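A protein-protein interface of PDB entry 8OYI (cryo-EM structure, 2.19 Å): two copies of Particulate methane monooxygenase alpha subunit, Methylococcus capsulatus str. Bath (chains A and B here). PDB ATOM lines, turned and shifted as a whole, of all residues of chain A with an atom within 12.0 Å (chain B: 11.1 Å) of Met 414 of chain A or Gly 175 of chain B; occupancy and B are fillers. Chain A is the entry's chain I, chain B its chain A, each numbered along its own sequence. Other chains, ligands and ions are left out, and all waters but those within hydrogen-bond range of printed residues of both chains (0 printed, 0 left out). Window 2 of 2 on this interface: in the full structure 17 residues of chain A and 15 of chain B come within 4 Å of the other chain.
The side-chain sulfur (SD) of Met 414 of chain A lies close to the backbone carbonyl oxygen (O) of Leu 173 of chain B.
Hydrophobic or aromatic side chains of chain A within 4 Å of the printed part of chain B: Ile 410, Phe 413 and Met 414.
Hydrophobic or aromatic side chains of chain B within 4 Å of the printed part of chain A: Leu 173 and Ile 260.
Among the printed residues, no Asp or Glu carboxylate lies within 4 Å of a Lys or Arg side-chain nitrogen of the other chain.
Met 414 of chain A touches three residues of chain B.
Of chain A, only Met 414 (3.9 Å) comes within 4 Å of Gly 175 of chain B.
No residue of chain B comes within 4 Å of Ser 412 of chain A.
No residue of chain A comes within 4 Å of Thr 171 of chain B.
Thr 172 of chain B touches none of the printed residues of chain A.
No residue of chain A comes within 4 Å of Gln 176 of chain B.
No residue of chain A comes within 4 Å of Thr 177 of chain B.
Of the printed residues of chain B, Phe 413 of chain A touches Leu 173 and Ile 260.
Printed residues of chain A within 4 Å of Leu 173 of chain B: Ile 410 (3.9 Å), Pro 411 (3.6 Å), Phe 413 (3.9 Å) and Met 414 (3.0 Å).
Ala 297 of chain A touches none of the printed residues of chain B.
The nearest residue of chain B that does not touch Met 414 of chain A is Thr 172 of chain B (5.7 Å).
The side-chain hydroxyl (OG1) of Thr 172 of chain B lies within hydrogen-bond range of the side-chain hydroxyl (OG1) of Thr 174 of chain B (2.5 Å).
The side-chain amide nitrogen (NE2) of Gln 176 of chain B is in hydrogen-bond range of the side-chain hydroxyl (OG1) of Thr 174 of chain B, at 3.3 Å.
The backbone carbonyl oxygen (O) of Ile 410 of chain A is in hydrogen-bond range of the backbone NH (N) of Tyr 291 of chain A.
O of Phe 413 of chain A lies within hydrogen-bond range of NH2 of Arg 292 of chain A, 2.7 Å away.
The backbone carbonyl oxygen of Met 414 of chain A lies within hydrogen-bond range of the guanidinium group of Arg 292 of chain A (2.4 Å).
No position is printed for both chains.
Of the 7 pairs that touch across the chains among the printed residues, none has its exchanged pair printed and touching as well.
Among the printed residues, merely in contact across the chains: Phe 413 of chain A with Ile 260 of chain B (3.4 Å), Pro 411 of chain A with Leu 173 of chain B (3.6 Å), Met 414 of chain A with Thr 174 of chain B (3.8 Å), Met 414 of chain A with Gly 175 of chain B (3.9 Å), Phe 413 of chain A with Leu 173 of chain B (3.9 Å) and Ile 410 of chain A with Leu 173 of chain B (3.9 Å).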
ATOM      1  N   THR A 290      -6.769  -7.948  15.204  1.00  0.00           N
ATOM      2  CA  THR A 290      -8.102  -8.226  14.695  1.00  0.00           C
ATOM      3  C   THR A 290      -8.132  -9.572  13.990  1.00  0.00           C
ATOM      4  O   THR A 290      -7.113 -10.057  13.491  1.00  0.00           O
ATOM      5  CB  THR A 290      -8.580  -7.132  13.726  1.00  0.00           C
ATOM      6  OG1 THR A 290      -7.644  -6.997  12.649  1.00  0.00           O
ATOM      7  CG2 THR A 290      -8.722  -5.796  14.443  1.00  0.00           C
ATOM      8  N   TYR A 291      -9.317 -10.174  13.968  1.00  0.00           N
ATOM      9  CA  TYR A 291      -9.566 -11.396  13.221  1.00  0.00           C
ATOM     10  C   TYR A 291     -10.936 -11.294  12.570  1.00  0.00           C
ATOM     11  O   TYR A 291     -11.879 -10.772  13.167  1.00  0.00           O
ATOM     12  CB  TYR A 291      -9.489 -12.639  14.118  1.00  0.00           C
ATOM     13  CG  TYR A 291     -10.594 -12.738  15.142  1.00  0.00           C
ATOM     14  CD1 TYR A 291     -10.644 -11.872  16.222  1.00  0.00           C
ATOM     15  CD2 TYR A 291     -11.591 -13.695  15.024  1.00  0.00           C
ATOM     16  CE1 TYR A 291     -11.647 -11.959  17.162  1.00  0.00           C
ATOM     17  CE2 TYR A 291     -12.600 -13.790  15.959  1.00  0.00           C
ATOM     18  CZ  TYR A 291     -12.622 -12.915  17.025  1.00  0.00           C
ATOM     19  OH  TYR A 291     -13.626 -13.002  17.960  1.00  0.00           O
ATOM     20  N   ARG A 292     -11.035 -11.787  11.339  1.00  0.00           N
ATOM     21  CA  ARG A 292     -12.282 -11.715  10.595  1.00  0.00           C
ATOM     22  C   ARG A 292     -13.256 -12.786  11.061  1.00  0.00           C
ATOM     23  O   ARG A 292     -12.870 -13.930  11.321  1.00  0.00           O
ATOM     24  CB  ARG A 292     -12.018 -11.871   9.097  1.00  0.00           C
ATOM     25  CG  ARG A 292     -11.132 -10.788   8.511  1.00  0.00           C
ATOM     26  CD  ARG A 292     -11.967  -9.639   7.987  1.00  0.00           C
ATOM     27  NE  ARG A 292     -13.351 -10.037   7.759  1.00  0.00           N
ATOM     28  CZ  ARG A 292     -14.391  -9.218   7.846  1.00  0.00           C
ATOM     29  NH1 ARG A 292     -14.240  -7.941   8.163  1.00  0.00           N
ATOM     30  NH2 ARG A 292     -15.611  -9.690   7.610  1.00  0.00           N
ATOM     31  N   VAL A 293     -14.526 -12.405  11.173  1.00  0.00           N
ATOM     32  CA  VAL A 293     -15.596 -13.341  11.508  1.00  0.00           C
ATOM     33  C   VAL A 293     -16.591 -13.372  10.350  1.00  0.00           C
ATOM     34  O   VAL A 293     -17.294 -12.379  10.115  1.00  0.00           O
ATOM     35  CB  VAL A 293     -16.292 -12.954  12.819  1.00  0.00           C
ATOM     36  CG1 VAL A 293     -17.247 -14.053  13.255  1.00  0.00           C
ATOM     37  CG2 VAL A 293     -15.266 -12.677  13.905  1.00  0.00           C
ATOM     38  N   PRO A 294     -16.684 -14.480   9.600  1.00  0.00           N
ATOM     39  CA  PRO A 294     -15.851 -15.673   9.753  1.00  0.00           C
ATOM     40  C   PRO A 294     -14.521 -15.542   9.019  1.00  0.00           C
ATOM     41  O   PRO A 294     -14.384 -14.687   8.144  1.00  0.00           O
ATOM     42  CB  PRO A 294     -16.704 -16.791   9.134  1.00  0.00           C
ATOM     43  CG  PRO A 294     -17.915 -16.103   8.512  1.00  0.00           C
ATOM     44  CD  PRO A 294     -17.647 -14.636   8.500  1.00  0.00           C
ATOM     45  N   GLY A 295     -13.561 -16.384   9.369  1.00  0.00           N
ATOM     46  CA  GLY A 295     -12.274 -16.363   8.697  1.00  0.00           C
ATOM     47  C   GLY A 295     -11.338 -17.367   9.325  1.00  0.00           C
ATOM     48  O   GLY A 295     -11.645 -17.993  10.345  1.00  0.00           O
ATOM     49  N   ALA A 297      -7.880 -16.353   9.578  1.00  0.00           N
ATOM     50  CA  ALA A 297      -6.691 -15.533   9.709  1.00  0.00           C
ATOM     51  C   ALA A 297      -6.830 -14.593  10.896  1.00  0.00           C
ATOM     52  O   ALA A 297      -7.931 -14.179  11.261  1.00  0.00           O
ATOM     53  CB  ALA A 297      -6.430 -14.718   8.437  1.00  0.00           C
ATOM     54  N   ARG A 299      -4.947 -10.967  12.322  1.00  0.00           N
ATOM     55  CA  ARG A 299      -4.107  -9.855  11.907  1.00  0.00           C
ATOM     56  C   ARG A 299      -3.775  -8.984  13.110  1.00  0.00           C
ATOM     57  O   ARG A 299      -4.647  -8.690  13.935  1.00  0.00           O
ATOM     58  CB  ARG A 299      -4.800  -9.019  10.827  1.00  0.00           C
ATOM     59  CG  ARG A 299      -3.885  -8.047  10.107  1.00  0.00           C
ATOM     60  CD  ARG A 299      -4.615  -6.751   9.794  1.00  0.00           C
ATOM     61  NE  ARG A 299      -5.185  -6.140  10.989  1.00  0.00           N
ATOM     62  CZ  ARG A 299      -4.478  -5.549  11.944  1.00  0.00           C
ATOM     63  NH1 ARG A 299      -3.163  -5.439  11.867  1.00  0.00           N
ATOM     64  NH2 ARG A 299      -5.112  -5.050  13.003  1.00  0.00           N
ATOM     65  N   ILE A 380     -14.789 -15.500  19.656  1.00  0.00           N
ATOM     66  CA  ILE A 380     -15.932 -14.595  19.639  1.00  0.00           C
ATOM     67  C   ILE A 380     -16.990 -15.041  20.642  1.00  0.00           C
ATOM     68  O   ILE A 380     -17.780 -14.223  21.127  1.00  0.00           O
ATOM     69  CB  ILE A 380     -16.503 -14.491  18.211  1.00  0.00           C
ATOM     70  CG1 ILE A 380     -17.420 -13.272  18.084  1.00  0.00           C
ATOM     71  CG2 ILE A 380     -17.229 -15.773  17.817  1.00  0.00           C
ATOM     72  CD1 ILE A 380     -18.236 -13.259  16.819  1.00  0.00           C
ATOM     73  N   ILE A 410      -9.827  -8.052  18.648  1.00  0.00           N
ATOM     74  CA  ILE A 410     -11.072  -7.396  18.263  1.00  0.00           C
ATOM     75  C   ILE A 410     -11.608  -8.077  17.008  1.00  0.00           C
ATOM     76  O   ILE A 410     -10.931  -8.051  15.971  1.00  0.00           O
ATOM     77  CB  ILE A 410     -10.867  -5.894  18.023  1.00  0.00           C
ATOM     78  CG1 ILE A 410     -10.237  -5.241  19.255  1.00  0.00           C
ATOM     79  CG2 ILE A 410     -12.182  -5.239  17.662  1.00  0.00           C
ATOM     80  CD1 ILE A 410     -11.040  -5.412  20.519  1.00  0.00           C
ATOM     81  N   PRO A 411     -12.792  -8.679  17.048  1.00  0.00           N
ATOM     82  CA  PRO A 411     -13.372  -9.231  15.823  1.00  0.00           C
ATOM     83  C   PRO A 411     -13.761  -8.138  14.844  1.00  0.00           C
ATOM     84  O   PRO A 411     -14.107  -7.017  15.224  1.00  0.00           O
ATOM     85  CB  PRO A 411     -14.605  -9.986  16.332  1.00  0.00           C
ATOM     86  CG  PRO A 411     -14.986  -9.262  17.578  1.00  0.00           C
ATOM     87  CD  PRO A 411     -13.690  -8.830  18.206  1.00  0.00           C
ATOM     88  N   SER A 412     -13.695  -8.478  13.560  1.00  0.00           N
ATOM     89  CA  SER A 412     -14.142  -7.600  12.485  1.00  0.00           C
ATOM     90  C   SER A 412     -15.154  -8.354  11.641  1.00  0.00           C
ATOM     91  O   SER A 412     -14.914  -9.504  11.262  1.00  0.00           O
ATOM     92  CB  SER A 412     -12.968  -7.127  11.624  1.00  0.00           C
ATOM     93  OG  SER A 412     -12.449  -8.188  10.843  1.00  0.00           O
ATOM     94  N   PHE A 413     -16.285  -7.713  11.352  1.00  0.00           N
ATOM     95  CA  PHE A 413     -17.391  -8.376  10.672  1.00  0.00           C
ATOM     96  C   PHE A 413     -17.640  -7.834   9.275  1.00  0.00           C
ATOM     97  O   PHE A 413     -17.999  -8.601   8.376  1.00  0.00           O
ATOM     98  CB  PHE A 413     -18.660  -8.269  11.532  1.00  0.00           C
ATOM     99  CG  PHE A 413     -18.443  -8.654  12.966  1.00  0.00           C
ATOM    100  CD1 PHE A 413     -18.443  -9.985  13.346  1.00  0.00           C
ATOM    101  CD2 PHE A 413     -18.226  -7.687  13.934  1.00  0.00           C
ATOM    102  CE1 PHE A 413     -18.236 -10.343  14.663  1.00  0.00           C
ATOM    103  CE2 PHE A 413     -18.020  -8.039  15.252  1.00  0.00           C
ATOM    104  CZ  PHE A 413     -18.024  -9.367  15.616  1.00  0.00           C
ATOM    105  N   MET A 414     -17.464  -6.534   9.061  1.00  0.00           N
ATOM    106  CA  MET A 414     -17.586  -5.970   7.720  1.00  0.00           C
ATOM    107  C   MET A 414     -16.215  -5.610   7.157  1.00  0.00           C
ATOM    108  O   MET A 414     -15.199  -5.745   7.838  1.00  0.00           O
ATOM    109  CB  MET A 414     -18.491  -4.733   7.720  1.00  0.00           C
ATOM    110  CG  MET A 414     -19.711  -4.850   8.611  1.00  0.00           C
ATOM    111  SD  MET A 414     -19.371  -4.335  10.301  1.00  0.00           S
ATOM    112  CE  MET A 414     -19.033  -2.592  10.064  1.00  0.00           C
ATOM    113  N   VAL B 170     -22.012   5.966  21.169  1.00  0.00           N
ATOM    114  CA  VAL B 170     -21.030   4.897  21.028  1.00  0.00           C
ATOM    115  C   VAL B 170     -21.242   4.236  19.676  1.00  0.00           C
ATOM    116  O   VAL B 170     -22.377   4.124  19.200  1.00  0.00           O
ATOM    117  CB  VAL B 170     -21.117   3.877  22.183  1.00  0.00           C
ATOM    118  CG1 VAL B 170     -22.385   3.046  22.091  1.00  0.00           C
ATOM    119  CG2 VAL B 170     -19.885   2.987  22.200  1.00  0.00           C
ATOM    120  N   THR B 171     -20.151   3.826  19.039  1.00  0.00           N
ATOM    121  CA  THR B 171     -20.216   3.170  17.743  1.00  0.00           C
ATOM    122  C   THR B 171     -19.846   1.702  17.898  1.00  0.00           C
ATOM    123  O   THR B 171     -18.790   1.371  18.446  1.00  0.00           O
ATOM    124  CB  THR B 171     -19.278   3.848  16.743  1.00  0.00           C
ATOM    125  OG1 THR B 171     -19.630   5.232  16.621  1.00  0.00           O
ATOM    126  CG2 THR B 171     -19.381   3.181  15.380  1.00  0.00           C
ATOM    127  N   THR B 172     -20.715   0.825  17.412  1.00  0.00           N
ATOM    128  CA  THR B 172     -20.510  -0.607  17.531  1.00  0.00           C
ATOM    129  C   THR B 172     -19.676  -1.128  16.365  1.00  0.00           C
ATOM    130  O   THR B 172     -19.462  -0.444  15.361  1.00  0.00           O
ATOM    131  CB  THR B 172     -21.850  -1.339  17.591  1.00  0.00           C
ATOM    132  OG1 THR B 172     -22.421  -1.393  16.281  1.00  0.00           O
ATOM    133  CG2 THR B 172     -22.808  -0.611  18.519  1.00  0.00           C
ATOM    134  N   LEU B 173     -19.201  -2.364  16.509  1.00  0.00           N
ATOM    135  CA  LEU B 173     -18.471  -3.013  15.428  1.00  0.00           C
ATOM    136  C   LEU B 173     -19.377  -3.408  14.273  1.00  0.00           C
ATOM    137  O   LEU B 173     -18.869  -3.813  13.220  1.00  0.00           O
ATOM    138  CB  LEU B 173     -17.727  -4.238  15.955  1.00  0.00           C
ATOM    139  CG  LEU B 173     -16.508  -3.928  16.823  1.00  0.00           C
ATOM    140  CD1 LEU B 173     -16.079  -5.153  17.603  1.00  0.00           C
ATOM    141  CD2 LEU B 173     -15.364  -3.411  15.966  1.00  0.00           C
ATOM    142  N   THR B 174     -20.695  -3.301  14.440  1.00  0.00           N
ATOM    143  CA  THR B 174     -21.631  -3.541  13.352  1.00  0.00           C
ATOM    144  C   THR B 174     -21.931  -2.281  12.553  1.00  0.00           C
ATOM    145  O   THR B 174     -22.774  -2.324  11.651  1.00  0.00           O
ATOM    146  CB  THR B 174     -22.939  -4.121  13.896  1.00  0.00           C
ATOM    147  OG1 THR B 174     -23.371  -3.352  15.023  1.00  0.00           O
ATOM    148  CG2 THR B 174     -22.734  -5.563  14.327  1.00  0.00           C
ATOM    149  N   GLY B 175     -21.275  -1.165  12.869  1.00  0.00           N
ATOM    150  CA  GLY B 175     -21.409   0.042  12.079  1.00  0.00           C
ATOM    151  C   GLY B 175     -22.612   0.904  12.377  1.00  0.00           C
ATOM    152  O   GLY B 175     -23.108   1.588  11.474  1.00  0.00           O
ATOM    153  N   GLN B 176     -23.100   0.904  13.613  1.00  0.00           N
ATOM    154  CA  GLN B 176     -24.213   1.761  13.992  1.00  0.00           C
ATOM    155  C   GLN B 176     -23.842   2.558  15.232  1.00  0.00           C
ATOM    156  O   GLN B 176     -23.168   2.046  16.130  1.00  0.00           O
ATOM    157  CB  GLN B 176     -25.488   0.951  14.252  1.00  0.00           C
ATOM    158  CG  GLN B 176     -25.262  -0.367  14.966  1.00  0.00           C
ATOM    159  CD  GLN B 176     -26.151  -1.472  14.432  1.00  0.00           C
ATOM    160  OE1 GLN B 176     -26.477  -1.501  13.245  1.00  0.00           O
ATOM    161  NE2 GLN B 176     -26.548  -2.387  15.305  1.00  0.00           N
ATOM    162  N   THR B 177     -24.282   3.811  15.271  1.00  0.00           N
ATOM    163  CA  THR B 177     -24.032   4.701  16.395  1.00  0.00           C
ATOM    164  C   THR B 177     -25.314   4.841  17.204  1.00  0.00           C
ATOM    165  O   THR B 177     -26.359   5.208  16.658  1.00  0.00           O
ATOM    166  CB  THR B 177     -23.550   6.071  15.916  1.00  0.00           C
ATOM    167  OG1 THR B 177     -22.290   5.928  15.251  1.00  0.00           O
ATOM    168  CG2 THR B 177     -23.391   7.018  17.097  1.00  0.00           C
ATOM    169  N   VAL B 178     -25.231   4.552  18.500  1.00  0.00           N
ATOM    170  CA  VAL B 178     -26.386   4.605  19.382  1.00  0.00           C
ATOM    171  C   VAL B 178     -26.056   5.489  20.576  1.00  0.00           C
ATOM    172  O   VAL B 178     -24.890   5.689  20.924  1.00  0.00           O
ATOM    173  CB  VAL B 178     -26.822   3.196  19.852  1.00  0.00           C
ATOM    174  CG1 VAL B 178     -26.911   2.242  18.675  1.00  0.00           C
ATOM    175  CG2 VAL B 178     -25.865   2.658  20.902  1.00  0.00           C
ATOM    176  N   TYR B 183     -30.838   3.908  24.281  1.00  0.00           N
ATOM    177  CA  TYR B 183     -30.776   2.744  23.406  1.00  0.00           C
ATOM    178  C   TYR B 183     -31.441   1.545  24.073  1.00  0.00           C
ATOM    179  O   TYR B 183     -31.211   1.273  25.255  1.00  0.00           O
ATOM    180  CB  TYR B 183     -29.320   2.429  23.067  1.00  0.00           C
ATOM    181  CG  TYR B 183     -29.099   1.120  22.354  1.00  0.00           C
ATOM    182  CD1 TYR B 183     -29.389   0.987  21.004  1.00  0.00           C
ATOM    183  CD2 TYR B 183     -28.584   0.018  23.026  1.00  0.00           C
ATOM    184  CE1 TYR B 183     -29.180  -0.205  20.345  1.00  0.00           C
ATOM    185  CE2 TYR B 183     -28.375  -1.179  22.375  1.00  0.00           C
ATOM    186  CZ  TYR B 183     -28.672  -1.285  21.035  1.00  0.00           C
ATOM    187  OH  TYR B 183     -28.463  -2.473  20.381  1.00  0.00           O
ATOM    188  N   TYR B 258     -29.780  -8.188  14.964  1.00  0.00           N
ATOM    189  CA  TYR B 258     -28.589  -8.354  15.792  1.00  0.00           C
ATOM    190  C   TYR B 258     -27.991  -9.753  15.621  1.00  0.00           C
ATOM    191  O   TYR B 258     -27.873 -10.505  16.592  1.00  0.00           O
ATOM    192  CB  TYR B 258     -28.896  -8.083  17.256  1.00  0.00           C
ATOM    193  CG  TYR B 258     -29.841  -6.935  17.500  1.00  0.00           C
ATOM    194  CD1 TYR B 258     -29.429  -5.622  17.344  1.00  0.00           C
ATOM    195  CD2 TYR B 258     -31.153  -7.168  17.887  1.00  0.00           C
ATOM    196  CE1 TYR B 258     -30.295  -4.572  17.564  1.00  0.00           C
ATOM    197  CE2 TYR B 258     -32.026  -6.124  18.109  1.00  0.00           C
ATOM    198  CZ  TYR B 258     -31.590  -4.829  17.947  1.00  0.00           C
ATOM    199  OH  TYR B 258     -32.456  -3.784  18.169  1.00  0.00           O
ATOM    200  N   PRO B 259     -27.612 -10.141  14.396  1.00  0.00           N
ATOM    201  CA  PRO B 259     -27.035 -11.477  14.212  1.00  0.00           C
ATOM    202  C   PRO B 259     -25.673 -11.637  14.864  1.00  0.00           C
ATOM    203  O   PRO B 259     -25.224 -12.772  15.053  1.00  0.00           O
ATOM    204  CB  PRO B 259     -26.942 -11.614  12.688  1.00  0.00           C
ATOM    205  CG  PRO B 259     -26.785 -10.218  12.208  1.00  0.00           C
ATOM    206  CD  PRO B 259     -27.546  -9.338  13.161  1.00  0.00           C
ATOM    207  N   ILE B 260     -25.009 -10.539  15.208  1.00  0.00           N
ATOM    208  CA  ILE B 260     -23.685 -10.567  15.809  1.00  0.00           C
ATOM    209  C   ILE B 260     -23.823 -10.101  17.254  1.00  0.00           C
ATOM    210  O   ILE B 260     -24.116  -8.929  17.514  1.00  0.00           O
ATOM    211  CB  ILE B 260     -22.692  -9.690  15.040  1.00  0.00           C
ATOM    212  CG1 ILE B 260     -22.423 -10.280  13.652  1.00  0.00           C
ATOM    213  CG2 ILE B 260     -21.406  -9.541  15.816  1.00  0.00           C
ATOM    214  CD1 ILE B 260     -22.690  -9.318  12.523  1.00  0.00           C
